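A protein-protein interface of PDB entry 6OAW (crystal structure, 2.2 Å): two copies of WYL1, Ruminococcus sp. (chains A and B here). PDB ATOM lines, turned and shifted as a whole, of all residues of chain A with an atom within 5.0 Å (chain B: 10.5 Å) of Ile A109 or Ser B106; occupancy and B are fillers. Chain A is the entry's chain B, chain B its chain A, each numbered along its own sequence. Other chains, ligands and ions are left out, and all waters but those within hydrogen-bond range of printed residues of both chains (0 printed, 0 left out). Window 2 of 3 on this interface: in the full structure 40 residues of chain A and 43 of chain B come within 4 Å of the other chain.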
ATOM      1  N   LYS A 105      35.411  18.005  13.675  1.00  0.00           N
ATOM      2  CA  LYS A 105      34.971  19.394  13.968  1.00  0.00           C
ATOM      3  C   LYS A 105      33.898  19.332  15.056  1.00  0.00           C
ATOM      4  O   LYS A 105      33.977  20.112  16.023  1.00  0.00           O
ATOM      5  CB  LYS A 105      34.498  20.099  12.692  1.00  0.00           C
ATOM      6  CG  LYS A 105      35.608  20.473  11.713  1.00  0.00           C
ATOM      7  N   SER A 106      32.950  18.402  14.932  1.00  0.00           N
ATOM      8  CA  SER A 106      31.874  18.202  15.940  1.00  0.00           C
ATOM      9  C   SER A 106      32.501  17.854  17.280  1.00  0.00           C
ATOM     10  O   SER A 106      32.096  18.446  18.271  1.00  0.00           O
ATOM     11  CB  SER A 106      30.866  17.173  15.512  1.00  0.00           C
ATOM     12  OG  SER A 106      30.170  17.665  14.385  1.00  0.00           O
ATOM     13  N   LYS A 107      33.446  16.924  17.306  1.00  0.00           N
ATOM     14  CA  LYS A 107      34.121  16.517  18.573  1.00  0.00           C
ATOM     15  C   LYS A 107      34.820  17.730  19.208  1.00  0.00           C
ATOM     16  O   LYS A 107      34.687  17.890  20.405  1.00  0.00           O
ATOM     17  CB  LYS A 107      35.141  15.404  18.334  1.00  0.00           C
ATOM     18  CG  LYS A 107      34.536  14.065  17.984  1.00  0.00           C
ATOM     19  CD  LYS A 107      35.568  12.963  17.824  1.00  0.00           C
ATOM     20  CE  LYS A 107      34.923  11.627  17.477  1.00  0.00           C
ATOM     21  NZ  LYS A 107      35.894  10.667  16.901  1.00  0.00           N
ATOM     22  N   GLU A 108      35.527  18.552  18.429  1.00  0.00           N
ATOM     23  CA  GLU A 108      36.234  19.751  18.969  1.00  0.00           C
ATOM     24  C   GLU A 108      35.197  20.692  19.614  1.00  0.00           C
ATOM     25  O   GLU A 108      35.440  21.204  20.739  1.00  0.00           O
ATOM     26  CB  GLU A 108      37.115  20.411  17.898  1.00  0.00           C
ATOM     27  CG  GLU A 108      38.356  19.571  17.542  1.00  0.00           C
ATOM     28  CD  GLU A 108      39.236  19.242  18.753  1.00  0.00           C
ATOM     29  OE1 GLU A 108      39.505  20.169  19.550  1.00  0.00           O
ATOM     30  OE2 GLU A 108      39.572  18.051  18.960  1.00  0.00           O
ATOM     31  N   ILE A 109      34.038  20.865  18.984  1.00  0.00           N
ATOM     32  CA  ILE A 109      32.971  21.721  19.567  1.00  0.00           C
ATOM     33  C   ILE A 109      32.445  21.087  20.862  1.00  0.00           C
ATOM     34  O   ILE A 109      32.220  21.828  21.837  1.00  0.00           O
ATOM     35  CB  ILE A 109      31.891  22.008  18.521  1.00  0.00           C
ATOM     36  CG1 ILE A 109      32.462  22.956  17.454  1.00  0.00           C
ATOM     37  CG2 ILE A 109      30.642  22.572  19.178  1.00  0.00           C
ATOM     38  CD1 ILE A 109      31.718  22.924  16.158  1.00  0.00           C
ATOM     39  N   ILE A 110      32.303  19.766  20.911  1.00  0.00           N
ATOM     40  CA  ILE A 110      31.782  19.098  22.129  1.00  0.00           C
ATOM     41  C   ILE A 110      32.854  19.219  23.217  1.00  0.00           C
ATOM     42  O   ILE A 110      32.494  19.503  24.373  1.00  0.00           O
ATOM     43  CB  ILE A 110      31.422  17.614  21.917  1.00  0.00           C
ATOM     44  CG1 ILE A 110      30.463  17.366  20.754  1.00  0.00           C
ATOM     45  CG2 ILE A 110      30.896  17.052  23.232  1.00  0.00           C
ATOM     46  CD1 ILE A 110      29.077  17.829  21.006  1.00  0.00           C
ATOM     47  N   LYS A 111      34.099  18.898  22.873  1.00  0.00           N
ATOM     48  CA  LYS A 111      35.276  19.020  23.772  1.00  0.00           C
ATOM     49  C   LYS A 111      35.304  20.411  24.423  1.00  0.00           C
ATOM     50  O   LYS A 111      35.369  20.453  25.643  1.00  0.00           O
ATOM     51  CB  LYS A 111      36.590  18.778  23.038  1.00  0.00           C
ATOM     52  CG  LYS A 111      36.994  17.323  22.817  1.00  0.00           C
ATOM     53  CD  LYS A 111      38.493  17.277  22.485  1.00  0.00           C
ATOM     54  CE  LYS A 111      38.919  16.068  21.677  1.00  0.00           C
ATOM     55  NZ  LYS A 111      40.284  16.297  21.148  1.00  0.00           N
ATOM     56  N   SER A 112      35.199  21.503  23.659  1.00  0.00           N
ATOM     57  CA  SER A 112      35.183  22.881  24.222  1.00  0.00           C
ATOM     58  C   SER A 112      33.967  23.070  25.141  1.00  0.00           C
ATOM     59  O   SER A 112      34.122  23.712  26.177  1.00  0.00           O
ATOM     60  CB  SER A 112      35.209  23.938  23.150  1.00  0.00           C
ATOM     61  OG  SER A 112      36.314  23.729  22.312  1.00  0.00           O
ATOM     62  N   TYR A 113      32.788  22.587  24.750  1.00  0.00           N
ATOM     63  CA  TYR A 113      31.566  22.681  25.584  1.00  0.00           C
ATOM     64  C   TYR A 113      31.818  21.999  26.934  1.00  0.00           C
ATOM     65  O   TYR A 113      31.389  22.559  27.954  1.00  0.00           O
ATOM     66  CB  TYR A 113      30.342  22.069  24.887  1.00  0.00           C
ATOM     67  CG  TYR A 113      29.211  21.685  25.816  1.00  0.00           C
ATOM     68  CD1 TYR A 113      28.281  22.630  26.239  1.00  0.00           C
ATOM     69  CD2 TYR A 113      29.070  20.396  26.306  1.00  0.00           C
ATOM     70  CE1 TYR A 113      27.236  22.307  27.090  1.00  0.00           C
ATOM     71  CE2 TYR A 113      28.038  20.059  27.172  1.00  0.00           C
ATOM     72  CZ  TYR A 113      27.100  21.011  27.551  1.00  0.00           C
ATOM     73  OH  TYR A 113      26.104  20.708  28.454  1.00  0.00           O
ATOM     74  N   ILE B  95      19.753  21.962  27.874  1.00  0.00           N
ATOM     75  CA  ILE B  95      19.775  22.590  26.517  1.00  0.00           C
ATOM     76  C   ILE B  95      19.961  24.110  26.683  1.00  0.00           C
ATOM     77  O   ILE B  95      20.869  24.634  26.080  1.00  0.00           O
ATOM     78  CB  ILE B  95      18.516  22.231  25.713  1.00  0.00           C
ATOM     79  CG1 ILE B  95      18.379  20.716  25.541  1.00  0.00           C
ATOM     80  CG2 ILE B  95      18.508  22.967  24.380  1.00  0.00           C
ATOM     81  CD1 ILE B  95      19.575  20.043  24.919  1.00  0.00           C
ATOM     82  N   ILE B  98      23.435  25.900  27.385  1.00  0.00           N
ATOM     83  CA  ILE B  98      24.456  26.015  26.312  1.00  0.00           C
ATOM     84  C   ILE B  98      24.812  27.500  26.126  1.00  0.00           C
ATOM     85  O   ILE B  98      23.914  28.332  25.964  1.00  0.00           O
ATOM     86  CB  ILE B  98      23.954  25.328  25.031  1.00  0.00           C
ATOM     87  CG1 ILE B  98      23.778  23.826  25.276  1.00  0.00           C
ATOM     88  CG2 ILE B  98      24.877  25.627  23.866  1.00  0.00           C
ATOM     89  CD1 ILE B  98      23.017  23.099  24.185  1.00  0.00           C
ATOM     90  N   ASP B  99      26.099  27.819  26.151  1.00  0.00           N
ATOM     91  CA  ASP B  99      26.593  29.216  26.013  1.00  0.00           C
ATOM     92  C   ASP B  99      25.854  29.902  24.858  1.00  0.00           C
ATOM     93  O   ASP B  99      26.041  29.494  23.693  1.00  0.00           O
ATOM     94  CB  ASP B  99      28.107  29.188  25.857  1.00  0.00           C
ATOM     95  CG  ASP B  99      28.753  30.547  25.717  1.00  0.00           C
ATOM     96  OD1 ASP B  99      28.009  31.539  25.540  1.00  0.00           O
ATOM     97  OD2 ASP B  99      29.995  30.583  25.808  1.00  0.00           O
ATOM     98  N   ASP B 100      25.037  30.904  25.173  1.00  0.00           N
ATOM     99  CA  ASP B 100      24.193  31.658  24.204  1.00  0.00           C
ATOM    100  C   ASP B 100      25.063  32.341  23.134  1.00  0.00           C
ATOM    101  O   ASP B 100      24.533  32.574  22.021  1.00  0.00           O
ATOM    102  CB  ASP B 100      23.331  32.710  24.920  1.00  0.00           C
ATOM    103  CG  ASP B 100      22.191  33.261  24.074  1.00  0.00           C
ATOM    104  N   SER B 101      26.340  32.640  23.427  1.00  0.00           N
ATOM    105  CA  SER B 101      27.242  33.373  22.504  1.00  0.00           C
ATOM    106  C   SER B 101      27.738  32.475  21.355  1.00  0.00           C
ATOM    107  O   SER B 101      28.329  33.033  20.412  1.00  0.00           O
ATOM    108  CB  SER B 101      28.399  33.987  23.244  1.00  0.00           C
ATOM    109  OG  SER B 101      29.288  32.983  23.736  1.00  0.00           O
ATOM    110  N   LEU B 102      27.551  31.147  21.415  1.00  0.00           N
ATOM    111  CA  LEU B 102      28.030  30.211  20.349  1.00  0.00           C
ATOM    112  C   LEU B 102      27.150  30.391  19.120  1.00  0.00           C
ATOM    113  O   LEU B 102      25.965  30.735  19.313  1.00  0.00           O
ATOM    114  CB  LEU B 102      27.981  28.764  20.847  1.00  0.00           C
ATOM    115  CG  LEU B 102      29.015  28.408  21.918  1.00  0.00           C
ATOM    116  CD1 LEU B 102      28.665  27.095  22.600  1.00  0.00           C
ATOM    117  CD2 LEU B 102      30.422  28.371  21.331  1.00  0.00           C
ATOM    118  N   ASP B 103      27.685  30.137  17.919  1.00  0.00           N
ATOM    119  CA  ASP B 103      26.877  30.174  16.668  1.00  0.00           C
ATOM    120  C   ASP B 103      25.844  29.044  16.692  1.00  0.00           C
ATOM    121  O   ASP B 103      25.952  28.107  17.542  1.00  0.00           O
ATOM    122  CB  ASP B 103      27.737  30.202  15.401  1.00  0.00           C
ATOM    123  CG  ASP B 103      28.894  29.224  15.266  1.00  0.00           C
ATOM    124  OD1 ASP B 103      28.738  28.059  15.684  1.00  0.00           O
ATOM    125  OD2 ASP B 103      29.934  29.635  14.658  1.00  0.00           O
ATOM    126  N   ASP B 104      24.817  29.175  15.853  1.00  0.00           N
ATOM    127  CA  ASP B 104      23.647  28.257  15.843  1.00  0.00           C
ATOM    128  C   ASP B 104      24.104  26.819  15.566  1.00  0.00           C
ATOM    129  O   ASP B 104      23.646  25.938  16.275  1.00  0.00           O
ATOM    130  CB  ASP B 104      22.601  28.706  14.825  1.00  0.00           C
ATOM    131  CG  ASP B 104      21.789  29.903  15.268  1.00  0.00           C
ATOM    132  OD1 ASP B 104      22.109  30.463  16.333  1.00  0.00           O
ATOM    133  OD2 ASP B 104      20.846  30.272  14.524  1.00  0.00           O
ATOM    134  N   LYS B 105      25.013  26.618  14.604  1.00  0.00           N
ATOM    135  CA  LYS B 105      25.523  25.273  14.247  1.00  0.00           C
ATOM    136  C   LYS B 105      26.157  24.593  15.474  1.00  0.00           C
ATOM    137  O   LYS B 105      25.819  23.448  15.739  1.00  0.00           O
ATOM    138  CB  LYS B 105      26.489  25.352  13.063  1.00  0.00           C
ATOM    139  CG  LYS B 105      26.991  24.001  12.576  1.00  0.00           C
ATOM    140  CD  LYS B 105      25.910  22.898  12.493  1.00  0.00           C
ATOM    141  CE  LYS B 105      25.300  22.747  11.117  1.00  0.00           C
ATOM    142  NZ  LYS B 105      24.201  21.743  11.165  1.00  0.00           N
ATOM    143  N   SER B 106      27.019  25.284  16.216  1.00  0.00           N
ATOM    144  CA  SER B 106      27.698  24.732  17.416  1.00  0.00           C
ATOM    145  C   SER B 106      26.651  24.327  18.450  1.00  0.00           C
ATOM    146  O   SER B 106      26.750  23.246  18.997  1.00  0.00           O
ATOM    147  CB  SER B 106      28.681  25.721  18.000  1.00  0.00           C
ATOM    148  OG  SER B 106      29.723  25.960  17.099  1.00  0.00           O
ATOM    149  N   LYS B 107      25.671  25.174  18.714  1.00  0.00           N
ATOM    150  CA  LYS B 107      24.590  24.855  19.681  1.00  0.00           C
ATOM    151  C   LYS B 107      23.804  23.614  19.232  1.00  0.00           C
ATOM    152  O   LYS B 107      23.554  22.737  20.088  1.00  0.00           O
ATOM    153  CB  LYS B 107      23.627  26.029  19.836  1.00  0.00           C
ATOM    154  CG  LYS B 107      24.243  27.255  20.494  1.00  0.00           C
ATOM    155  CD  LYS B 107      23.494  28.512  20.140  1.00  0.00           C
ATOM    156  CE  LYS B 107      23.494  29.539  21.245  1.00  0.00           C
ATOM    157  NZ  LYS B 107      22.603  30.653  20.860  1.00  0.00           N
ATOM    158  N   GLU B 108      23.434  23.524  17.952  1.00  0.00           N
ATOM    159  CA  GLU B 108      22.702  22.344  17.405  1.00  0.00           C
ATOM    160  C   GLU B 108      23.573  21.095  17.608  1.00  0.00           C
ATOM    161  O   GLU B 108      23.048  20.074  18.024  1.00  0.00           O
ATOM    162  CB  GLU B 108      22.315  22.548  15.932  1.00  0.00           C
ATOM    163  CG  GLU B 108      21.254  23.619  15.705  1.00  0.00           C
ATOM    164  CD  GLU B 108      19.942  23.374  16.433  1.00  0.00           C
ATOM    165  OE1 GLU B 108      19.397  22.242  16.316  1.00  0.00           O
ATOM    166  OE2 GLU B 108      19.496  24.297  17.169  1.00  0.00           O
ATOM    167  N   ILE B 109      24.886  21.184  17.400  1.00  0.00           N
ATOM    168  CA  ILE B 109      25.801  20.020  17.589  1.00  0.00           C
ATOM    169  C   ILE B 109      25.800  19.645  19.068  1.00  0.00           C
ATOM    170  O   ILE B 109      25.779  18.441  19.358  1.00  0.00           O
ATOM    171  CB  ILE B 109      27.211  20.307  17.047  1.00  0.00           C
ATOM    172  CG1 ILE B 109      27.182  20.315  15.520  1.00  0.00           C
ATOM    173  CG2 ILE B 109      28.231  19.324  17.591  1.00  0.00           C
ATOM    174  CD1 ILE B 109      28.344  21.033  14.911  1.00  0.00           C
ATOM    175  N   ILE B 110      25.819  20.623  19.971  1.00  0.00           N
ATOM    176  CA  ILE B 110      25.875  20.292  21.418  1.00  0.00           C
ATOM    177  C   ILE B 110      24.520  19.717  21.822  1.00  0.00           C
ATOM    178  O   ILE B 110      24.526  18.749  22.565  1.00  0.00           O
ATOM    179  CB  ILE B 110      26.307  21.492  22.269  1.00  0.00           C
ATOM    180  CG1 ILE B 110      27.703  21.984  21.859  1.00  0.00           C
ATOM    181  CG2 ILE B 110      26.237  21.130  23.730  1.00  0.00           C
ATOM    182  CD1 ILE B 110      27.951  23.444  22.106  1.00  0.00           C
ATOM    183  N   LYS B 111      23.420  20.334  21.382  1.00  0.00           N
ATOM    184  CA  LYS B 111      22.026  19.869  21.638  1.00  0.00           C
ATOM    185  C   LYS B 111      21.919  18.387  21.254  1.00  0.00           C
ATOM    186  O   LYS B 111      21.481  17.607  22.096  1.00  0.00           O
ATOM    187  CB  LYS B 111      20.983  20.661  20.841  1.00  0.00           C
ATOM    188  CG  LYS B 111      20.549  22.001  21.439  1.00  0.00           C
ATOM    189  CD  LYS B 111      19.443  22.743  20.639  1.00  0.00           C
ATOM    190  CE  LYS B 111      19.632  24.256  20.595  1.00  0.00           C
ATOM    191  N   SER B 112      22.325  18.011  20.038  1.00  0.00           N
ATOM    192  CA  SER B 112      22.256  16.608  19.550  1.00  0.00           C
ATOM    193  C   SER B 112      23.146  15.709  20.407  1.00  0.00           C
ATOM    194  O   SER B 112      22.688  14.590  20.723  1.00  0.00           O
ATOM    195  CB  SER B 112      22.604  16.496  18.100  1.00  0.00           C
ATOM    196  OG  SER B 112      21.706  17.299  17.370  1.00  0.00           O
ATOM    197  N   TYR B 113      24.357  16.157  20.751  1.00  0.00           N
ATOM    198  CA  TYR B 113      25.262  15.392  21.648  1.00  0.00           C
ATOM    199  C   TYR B 113      24.558  15.125  22.984  1.00  0.00           C
ATOM    200  O   TYR B 113      24.708  14.029  23.488  1.00  0.00           O
ATOM    201  CB  TYR B 113      26.579  16.122  21.905  1.00  0.00           C
ATOM    202  CG  TYR B 113      27.321  15.734  23.154  1.00  0.00           C
ATOM    203  CD1 TYR B 113      28.177  14.652  23.179  1.00  0.00           C
ATOM    204  CD2 TYR B 113      27.218  16.491  24.300  1.00  0.00           C
ATOM    205  CE1 TYR B 113      28.899  14.321  24.315  1.00  0.00           C
ATOM    206  CE2 TYR B 113      27.929  16.178  25.456  1.00  0.00           C
ATOM    207  CZ  TYR B 113      28.765  15.076  25.464  1.00  0.00           C
ATOM    208  OH  TYR B 113      29.464  14.742  26.589  1.00  0.00           O
ATOM    209  N   LEU B 114      23.870  16.109  23.558  1.00  0.00           N
ATOM    210  CA  LEU B 114      23.212  15.959  24.880  1.00  0.00           C
ATOM    211  C   LEU B 114      21.998  15.017  24.783  1.00  0.00           C
ATOM    212  O   LEU B 114      21.868  14.144  25.640  1.00  0.00           O
ATOM    213  CB  LEU B 114      22.819  17.330  25.434  1.00  0.00           C
ATOM    214  CG  LEU B 114      23.940  18.058  26.176  1.00  0.00           C
ATOM    215  CD1 LEU B 114      23.558  19.501  26.479  1.00  0.00           C
ATOM    216  CD2 LEU B 114      24.283  17.331  27.468  1.00  0.00           C
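The side-chain carboxylate (OD1) of Asp B103 is in hydrogen-bond range of the side-chain hydroxyl (OG) of Ser B106 (2.7 Å).
Among the printed residues, pairs that only touch across the chains: Ile A110 with Tyr B113 (3.2 Å), Tyr A113 with Leu B114 (3.4 Å), Tyr A113 with Ile B110 (3.6 Å), Ile A110 with Ile B109 (3.7 Å), Ile A109 with Ser B106 (3.8 Å) and Ser A106 with Ile B109 (3.9 Å).
No residue of chain B comes within 4 Å of Lys A105.
Ser A106 touches just one residue of chain B: Ile B109 (3.9 Å).
No residue of chain B comes within 4 Å of Glu A108.
Of chain B, only Ser B106 comes within 4 Å of Ile A109.
Ile A110 touches two residues of chain B.
Printed residues of chain B within 4 Å of Tyr A113: Ile B110 (3.6 Å) and Leu B114 (3.4 Å).
Leu B102 touches none of the printed residues of chain A.
Of the printed residues of chain A, Ser B106 touches Ile A109 (3.8 Å).
Of the printed residues of chain A, Ile B109 touches Ser A106 and Ile A110.
Printed residues of chain A within 4 Å of Ile B110: Tyr A113.
Lys B111 touches none of the printed residues of chain A.
Of the printed residues of chain A, Tyr B113 touches Ile A110 (3.2 Å).
Of the printed residues of chain A, Leu B114 touches Tyr A113 (3.4 Å).
The nearest printed residue of chain A that does not touch Ser B106 is Ile A110 (6.2 Å).
The nearest printed residue of chain B that does not touch Tyr A113 is Ile B98 (4.2 Å).
Of the 9 printed residues of chain A, 4 touch a printed residue of chain B.
Hydrophobic or aromatic side chains of chain A that line the printed part of chain B: Ile A109, Ile A110 and Tyr A113.
Of the 18 printed residues of chain B, 5 touch a printed residue of chain A.
Printed residues of chain B that touch a printed residue of chain A: Ser B106, Ile B109, Ile B110, Tyr B113 and Leu B114.
Hydrophobic or aromatic side chains of chain B that line the printed part of chain A: Ile B109, Ile B110, Tyr B113 and Leu B114.
Among the printed residues, 6 pairs touch across the chains.
Ser A106 touches Ile B109, and with the chains exchanged Ile A109 touches Ser B106.
Ile A110 touches Ile B109, but with the chains exchanged Ile A109 does not touch Ile B110 (4.02 Å).
Ile A110 touches Tyr B113, and with the chains exchanged Tyr A113 touches Ile B110.
Of the 6 pairs that touch across the chains among the printed residues, 4 have their exchanged pair printed and touching as well.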
